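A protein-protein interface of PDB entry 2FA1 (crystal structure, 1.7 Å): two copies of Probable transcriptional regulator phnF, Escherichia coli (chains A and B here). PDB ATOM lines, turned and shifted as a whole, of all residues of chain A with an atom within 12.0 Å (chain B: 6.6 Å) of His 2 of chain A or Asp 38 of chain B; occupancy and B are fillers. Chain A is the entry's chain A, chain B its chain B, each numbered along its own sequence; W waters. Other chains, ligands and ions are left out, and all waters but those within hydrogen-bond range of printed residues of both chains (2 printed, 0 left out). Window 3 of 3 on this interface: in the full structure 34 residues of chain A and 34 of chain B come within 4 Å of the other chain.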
ATOM      1  N   HIS A   2       6.374  10.113  23.268  1.00  0.00           N
ATOM      2  CA  HIS A   2       6.831  11.436  22.723  1.00  0.00           C
ATOM      3  C   HIS A   2       6.688  11.466  21.184  1.00  0.00           C
ATOM      4  O   HIS A   2       6.986  10.484  20.494  1.00  0.00           O
ATOM      5  CB  HIS A   2       8.305  11.674  23.179  1.00  0.00           C
ATOM      6  N   MET A   3       6.227  12.586  20.631  1.00  0.00           N
ATOM      7  CA  MET A   3       6.036  12.670  19.170  1.00  0.00           C
ATOM      8  C   MET A   3       7.270  13.167  18.389  1.00  0.00           C
ATOM      9  O   MET A   3       7.967  14.096  18.813  1.00  0.00           O
ATOM     10  CB  MET A   3       4.809  13.557  18.826  1.00  0.00           C
ATOM     11  CG  MET A   3       3.481  12.996  19.370  1.00  0.00           C
ATOM     12  SD  MET A   3       2.108  14.139  19.043  1.00  0.00           S
ATOM     13  CE  MET A   3       2.271  15.307  20.295  1.00  0.00           C
ATOM     14  N   ASN A   4       7.544  12.541  17.264  1.00  0.00           N
ATOM     15  CA  ASN A   4       8.576  13.066  16.423  1.00  0.00           C
ATOM     16  C   ASN A   4       8.124  14.431  15.904  1.00  0.00           C
ATOM     17  O   ASN A   4       6.949  14.767  15.974  1.00  0.00           O
ATOM     18  CB  ASN A   4       8.901  12.104  15.288  1.00  0.00           C
ATOM     19  CG  ASN A   4       7.724  11.824  14.388  1.00  0.00           C
ATOM     20  OD1 ASN A   4       7.881  11.771  13.187  1.00  0.00           O
ATOM     21  ND2 ASN A   4       6.553  11.615  14.959  1.00  0.00           N
ATOM     22  N   ALA A   5       9.075  15.194  15.390  1.00  0.00           N
ATOM     23  CA  ALA A   5       8.798  16.522  14.762  1.00  0.00           C
ATOM     24  C   ALA A   5       8.709  16.380  13.239  1.00  0.00           C
ATOM     25  O   ALA A   5       9.528  15.683  12.671  1.00  0.00           O
ATOM     26  CB  ALA A   5       9.888  17.461  15.157  1.00  0.00           C
ATOM     27  N   GLN A   6       7.701  16.993  12.594  1.00  0.00           N
ATOM     28  CA  GLN A   6       7.442  16.906  11.156  1.00  0.00           C
ATOM     29  C   GLN A   6       8.116  18.042  10.392  1.00  0.00           C
ATOM     30  O   GLN A   6       7.941  18.175   9.170  1.00  0.00           O
ATOM     31  CB  GLN A   6       5.928  17.030  10.837  1.00  0.00           C
ATOM     32  CG  GLN A   6       5.069  15.891  11.327  1.00  0.00           C
ATOM     33  CD  GLN A   6       3.945  15.537  10.365  1.00  0.00           C
ATOM     34  OE1 GLN A   6       3.569  14.355  10.245  1.00  0.00           O
ATOM     35  NE2 GLN A   6       3.378  16.563   9.682  1.00  0.00           N
ATOM     36  N   SER A  10      10.555  23.769  15.841  1.00  0.00           N
ATOM     37  CA  SER A  10       9.263  23.713  16.622  1.00  0.00           C
ATOM     38  C   SER A  10       9.032  25.021  17.325  1.00  0.00           C
ATOM     39  O   SER A  10       9.979  25.596  17.891  1.00  0.00           O
ATOM     40  CB  SER A  10       9.254  22.614  17.715  1.00  0.00           C
ATOM     41  OG  SER A  10       9.384  21.316  17.161  1.00  0.00           O
ATOM     42  N   GLU A 155       6.755  23.576  12.794  1.00  0.00           N
ATOM     43  CA  GLU A 155       5.565  22.916  13.349  1.00  0.00           C
ATOM     44  C   GLU A 155       5.276  23.549  14.720  1.00  0.00           C
ATOM     45  O   GLU A 155       6.198  24.016  15.423  1.00  0.00           O
ATOM     46  CB  GLU A 155       5.855  21.392  13.418  1.00  0.00           C
ATOM     47  CG  GLU A 155       4.929  20.586  14.354  1.00  0.00           C
ATOM     48  CD  GLU A 155       5.140  19.082  14.210  1.00  0.00           C
ATOM     49  OE1 GLU A 155       6.269  18.640  14.519  1.00  0.00           O
ATOM     50  OE2 GLU A 155       4.199  18.315  13.822  1.00  0.00           O
ATOM     51  N   THR A 157       3.754  23.468  18.640  1.00  0.00           N
ATOM     52  CA  THR A 157       3.515  22.470  19.692  1.00  0.00           C
ATOM     53  C   THR A 157       2.662  23.103  20.790  1.00  0.00           C
ATOM     54  O   THR A 157       2.688  24.314  20.969  1.00  0.00           O
ATOM     55  CB  THR A 157       4.860  21.969  20.330  1.00  0.00           C
ATOM     56  OG1 THR A 157       5.571  23.093  20.843  1.00  0.00           O
ATOM     57  CG2 THR A 157       5.708  21.287  19.258  1.00  0.00           C
ATOM     58  N   MET A 158       1.976  22.286  21.578  1.00  0.00           N
ATOM     59  CA  MET A 158       1.270  22.865  22.725  1.00  0.00           C
ATOM     60  C   MET A 158       1.272  21.819  23.828  1.00  0.00           C
ATOM     61  O   MET A 158       1.125  20.618  23.556  1.00  0.00           O
ATOM     62  CB  MET A 158      -0.143  23.326  22.311  1.00  0.00           C
ATOM     63  CG  MET A 158      -1.130  23.551  23.427  1.00  0.00           C
ATOM     64  SD  MET A 158      -2.542  24.369  22.711  1.00  0.00           S
ATOM     65  CE  MET A 158      -2.607  23.453  21.178  1.00  0.00           C
ATOM     66  N   GLU A 159       1.567  22.271  25.044  1.00  0.00           N
ATOM     67  CA  GLU A 159       1.559  21.353  26.215  1.00  0.00           C
ATOM     68  C   GLU A 159       0.292  21.650  26.961  1.00  0.00           C
ATOM     69  O   GLU A 159      -0.128  22.833  27.101  1.00  0.00           O
ATOM     70  CB  GLU A 159       2.733  21.644  27.148  1.00  0.00           C
ATOM     71  CG  GLU A 159       4.081  21.409  26.514  1.00  0.00           C
ATOM     72  CD  GLU A 159       4.396  19.962  26.442  1.00  0.00           C
ATOM     73  OE1 GLU A 159       3.798  19.215  27.256  1.00  0.00           O
ATOM     74  OE2 GLU A 159       5.223  19.570  25.576  1.00  0.00           O
ATOM     75  N   SER B  33       4.147   0.922  13.665  1.00  0.00           N
ATOM     76  CA  SER B  33       5.269   1.586  12.970  1.00  0.00           C
ATOM     77  C   SER B  33       6.235   2.210  13.957  1.00  0.00           C
ATOM     78  O   SER B  33       5.947   2.328  15.174  1.00  0.00           O
ATOM     79  CB  SER B  33       4.751   2.625  11.964  1.00  0.00           C
ATOM     80  OG  SER B  33       4.141   3.715  12.643  1.00  0.00           O
ATOM     81  N   GLY B  34       7.417   2.625  13.475  1.00  0.00           N
ATOM     82  CA  GLY B  34       8.375   3.214  14.410  1.00  0.00           C
ATOM     83  C   GLY B  34       7.854   4.522  14.981  1.00  0.00           C
ATOM     84  O   GLY B  34       8.085   4.844  16.128  1.00  0.00           O
ATOM     85  N   HIS B  35       7.103   5.273  14.195  1.00  0.00           N
ATOM     86  CA  HIS B  35       6.614   6.580  14.627  1.00  0.00           C
ATOM     87  C   HIS B  35       5.453   6.413  15.660  1.00  0.00           C
ATOM     88  O   HIS B  35       5.394   7.136  16.664  1.00  0.00           O
ATOM     89  CB  HIS B  35       6.263   7.383  13.375  1.00  0.00           C
ATOM     90  CG  HIS B  35       4.926   8.051  13.387  1.00  0.00           C
ATOM     91  ND1 HIS B  35       3.822   7.519  12.737  1.00  0.00           N
ATOM     92  CD2 HIS B  35       4.531   9.252  13.878  1.00  0.00           C
ATOM     93  CE1 HIS B  35       2.800   8.347  12.863  1.00  0.00           C
ATOM     94  NE2 HIS B  35       3.211   9.417  13.527  1.00  0.00           N
ATOM     95  N   VAL B  36       4.589   5.436  15.421  1.00  0.00           N
ATOM     96  CA  VAL B  36       3.540   5.085  16.428  1.00  0.00           C
ATOM     97  C   VAL B  36       4.098   4.545  17.734  1.00  0.00           C
ATOM     98  O   VAL B  36       3.711   4.972  18.864  1.00  0.00           O
ATOM     99  CB  VAL B  36       2.477   4.165  15.773  1.00  0.00           C
ATOM    100  CG1 VAL B  36       1.515   3.561  16.840  1.00  0.00           C
ATOM    101  CG2 VAL B  36       1.736   5.046  14.802  1.00  0.00           C
ATOM    102  N   ALA B  37       5.049   3.628  17.586  1.00  0.00           N
ATOM    103  CA  ALA B  37       5.742   3.082  18.737  1.00  0.00           C
ATOM    104  C   ALA B  37       6.425   4.158  19.581  1.00  0.00           C
ATOM    105  O   ALA B  37       6.274   4.173  20.806  1.00  0.00           O
ATOM    106  CB  ALA B  37       6.711   1.987  18.297  1.00  0.00           C
ATOM    107  N   ASP B  38       7.135   5.115  18.957  1.00  0.00           N
ATOM    108  CA  ASP B  38       7.688   6.220  19.732  1.00  0.00           C
ATOM    109  C   ASP B  38       6.716   7.090  20.438  1.00  0.00           C
ATOM    110  O   ASP B  38       6.990   7.535  21.545  1.00  0.00           O
ATOM    111  CB  ASP B  38       8.592   7.098  18.879  1.00  0.00           C
ATOM    112  CG  ASP B  38      10.023   6.549  18.826  1.00  0.00           C
ATOM    113  OD1 ASP B  38      10.901   7.093  19.562  1.00  0.00           O
ATOM    114  OD2 ASP B  38      10.251   5.547  18.096  1.00  0.00           O
ATOM    115  N   ALA B  39       5.598   7.454  19.777  1.00  0.00           N
ATOM    116  CA  ALA B  39       4.624   8.261  20.472  1.00  0.00           C
ATOM    117  C   ALA B  39       4.043   7.575  21.695  1.00  0.00           C
ATOM    118  O   ALA B  39       3.813   8.224  22.694  1.00  0.00           O
ATOM    119  CB  ALA B  39       3.460   8.674  19.500  1.00  0.00           C
ATOM    120  N   LEU B  40       3.725   6.287  21.564  1.00  0.00           N
ATOM    121  CA  LEU B  40       3.056   5.508  22.623  1.00  0.00           C
ATOM    122  C   LEU B  40       4.005   5.033  23.739  1.00  0.00           C
ATOM    123  O   LEU B  40       3.558   4.485  24.733  1.00  0.00           O
ATOM    124  CB  LEU B  40       2.346   4.287  22.036  1.00  0.00           C
ATOM    125  CG  LEU B  40       1.033   4.681  21.302  1.00  0.00           C
ATOM    126  CD1 LEU B  40       0.317   3.565  20.612  1.00  0.00           C
ATOM    127  CD2 LEU B  40       0.120   5.453  22.178  1.00  0.00           C
ATOM    128  N   GLY B  41       5.297   5.189  23.509  1.00  0.00           N
ATOM    129  CA  GLY B  41       6.318   4.627  24.410  1.00  0.00           C
ATOM    130  C   GLY B  41       6.351   3.108  24.383  1.00  0.00           C
ATOM    131  O   GLY B  41       6.476   2.454  25.464  1.00  0.00           O
ATOM    132  N   ILE B  42       6.293   2.514  23.187  1.00  0.00           N
ATOM    133  CA  ILE B  42       6.259   1.043  23.084  1.00  0.00           C
ATOM    134  C   ILE B  42       7.273   0.536  22.060  1.00  0.00           C
ATOM    135  O   ILE B  42       8.078   1.308  21.548  1.00  0.00           O
ATOM    136  CB  ILE B  42       4.848   0.480  22.774  1.00  0.00           C
ATOM    137  CG1 ILE B  42       4.368   0.946  21.378  1.00  0.00           C
ATOM    138  CG2 ILE B  42       3.865   0.885  23.866  1.00  0.00           C
ATOM    139  CD1 ILE B  42       3.204   0.132  20.830  1.00  0.00           C
ATOM    140  N   THR B  43       7.217  -0.762  21.778  1.00  0.00           N
ATOM    141  CA  THR B  43       8.145  -1.430  20.907  1.00  0.00           C
ATOM    142  C   THR B  43       7.621  -1.524  19.472  1.00  0.00           C
ATOM    143  O   THR B  43       6.524  -2.081  19.198  1.00  0.00           O
ATOM    144  CB  THR B  43       8.551  -2.859  21.449  1.00  0.00           C
ATOM    145  OG1 THR B  43       8.865  -2.787  22.850  1.00  0.00           O
ATOM    146  CG2 THR B  43       9.761  -3.362  20.724  1.00  0.00           C
ATOM    147  N   GLU B  44       8.417  -1.009  18.541  1.00  0.00           N
ATOM    148  CA  GLU B  44       8.157  -1.262  17.099  1.00  0.00           C
ATOM    149  C   GLU B  44       7.768  -2.692  16.709  1.00  0.00           C
ATOM    150  O   GLU B  44       8.477  -3.683  16.974  1.00  0.00           O
ATOM    151  CB  GLU B  44       9.281  -0.758  16.198  1.00  0.00           C
ATOM    152  CG  GLU B  44       9.008  -0.982  14.681  1.00  0.00           C
ATOM    153  CD  GLU B  44       9.930  -0.171  13.802  1.00  0.00           C
ATOM    154  OE1 GLU B  44      10.605   0.747  14.339  1.00  0.00           O
ATOM    155  OE2 GLU B  44       9.985  -0.434  12.570  1.00  0.00           O
ATOM    156  N   GLN B 102      -0.250  16.499  24.903  1.00  0.00           N
ATOM    157  CA  GLN B 102       0.561  17.278  23.958  1.00  0.00           C
ATOM    158  C   GLN B 102      -0.118  17.344  22.614  1.00  0.00           C
ATOM    159  O   GLN B 102      -0.773  16.416  22.188  1.00  0.00           O
ATOM    160  CB  GLN B 102       1.874  16.598  23.754  1.00  0.00           C
ATOM    161  CG  GLN B 102       2.821  17.012  24.863  1.00  0.00           C
ATOM    162  CD  GLN B 102       3.962  16.060  25.071  1.00  0.00           C
ATOM    163  OE1 GLN B 102       4.246  15.204  24.232  1.00  0.00           O
ATOM    164  NE2 GLN B 102       4.643  16.217  26.207  1.00  0.00           N
ATOM    165  N   LEU B 132      -1.281  13.391  21.785  1.00  0.00           N
ATOM    166  CA  LEU B 132      -1.118  12.285  22.736  1.00  0.00           C
ATOM    167  C   LEU B 132      -2.116  12.545  23.821  1.00  0.00           C
ATOM    168  O   LEU B 132      -2.196  13.671  24.396  1.00  0.00           O
ATOM    169  CB  LEU B 132       0.317  12.226  23.324  1.00  0.00           C
ATOM    170  CG  LEU B 132       1.382  11.795  22.323  1.00  0.00           C
ATOM    171  CD1 LEU B 132       2.780  11.914  23.020  1.00  0.00           C
ATOM    172  CD2 LEU B 132       1.215  10.369  21.751  1.00  0.00           C
ATOM    173  N   PRO B 141       0.973   7.818  27.604  1.00  0.00           N
ATOM    174  CA  PRO B 141      -0.084   8.061  26.621  1.00  0.00           C
ATOM    175  C   PRO B 141      -0.912   6.829  26.313  1.00  0.00           C
ATOM    176  O   PRO B 141      -0.366   5.789  25.962  1.00  0.00           O
ATOM    177  CB  PRO B 141       0.685   8.525  25.358  1.00  0.00           C
ATOM    178  CG  PRO B 141       2.104   8.116  25.592  1.00  0.00           C
ATOM    179  CD  PRO B 141       2.318   8.108  27.069  1.00  0.00           C
HETATM  180  O   HOH W   1       5.623  14.527  22.311  1.00  0.00           O
HETATM  181  O   HOH W   2       6.231   9.488  16.548  1.00  0.00           O
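Hydrophobic or aromatic side chains of chain A that line the printed part of chain B: Met 3.
Printed residues of chain B that touch a printed residue of chain A: His 35, Asp 38, Ala 39, Gln 102 and Leu 132.
Hydrophobic or aromatic side chains of chain B that line the printed part of chain A: His 35 and Leu 132.
Among the printed residues, no Asp or Glu carboxylate lies within 4 Å of a Lys or Arg side-chain nitrogen of the other chain.
The backbone carbonyl oxygen (O) of Gln 102 of chain B sits at hydrogen-bond distance from the backbone NH (N) of Leu 132 of chain B, at 3.1 Å.
No position is printed for both chains.
Of the 7 pairs that touch across the chains among the printed residues, none has its exchanged pair printed and touching as well.
The side-chain carboxylate of Glu 159 of chain A is in hydrogen-bond range of the side-chain amide nitrogen of Gln 102 of chain B (3.3 Å).
The backbone NH (N) of His 2 of chain A sits at hydrogen-bond distance from the backbone carbonyl oxygen (O) of Ala 39 of chain B, at 3.2 Å.
N of His 2 of chain A is in hydrogen-bond range of O of Asp 38 of chain B (3.2 Å).
Water W1 lies within hydrogen-bond range of OE1 of Gln 102 of chain B (2.5 Å) and N of Met 3 of chain A (2.6 Å).
Water W2 bridges the backbone carbonyl oxygen (O) of His 35 of chain B (2.5 Å) and the side-chain amide nitrogen (ND2) of Asn 4 of chain A (2.7 Å).
His 2 of chain A touches just these residues of chain B: Asp 38 (3.1 Å) and Ala 39 (3.2 Å).
Printed residues of chain B within 4 Å of Met 3 of chain A: Gln 102 and Leu 132.
Of the printed residues of chain B, Glu 159 of chain A touches Gln 102.
No residue of chain A comes within 4 Å of Ser 33 of chain B.
Printed residues of chain A within 4 Å of His 35 of chain B: Asn 4 (3.3 Å).
Val 36 of chain B touches none of the printed residues of chain A.
Printed residues of chain A within 4 Å of Asp 38 of chain B: His 2 (3.1 Å).
Of chain A, only His 2 (3.2 Å) comes within 4 Å of Ala 39 of chain B.
No residue of chain A comes within 4 Å of Leu 40 of chain B.
No residue of chain A comes within 4 Å of Gly 41 of chain B.
No residue of chain A comes within 4 Å of Ile 42 of chain B.
Of the printed residues of chain A, Gln 102 of chain B touches Met 3 (3.7 Å), Met 158 (3.4 Å) and Glu 159 (3.3 Å).
Of the printed residues of chain A, Leu 132 of chain B touches Met 3 (3.8 Å).
The nearest residue of chain B that does not touch His 2 of chain A is Leu 132 of chain B (4.03 Å).
The nearest printed residue of chain B that does not touch Asn 4 of chain A is Asp 38 of chain B (5.8 Å).
Among the printed residues, pairs that only touch across the chains: Met 3 of chain A with Gln 102 of chain B (3.7 Å), Met 3 of chain A with Leu 132 of chain B (3.8 Å), Asn 4 of chain A with His 35 of chain B (3.3 Å) and Met 158 of chain A with Gln 102 of chain B (3.4 Å).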
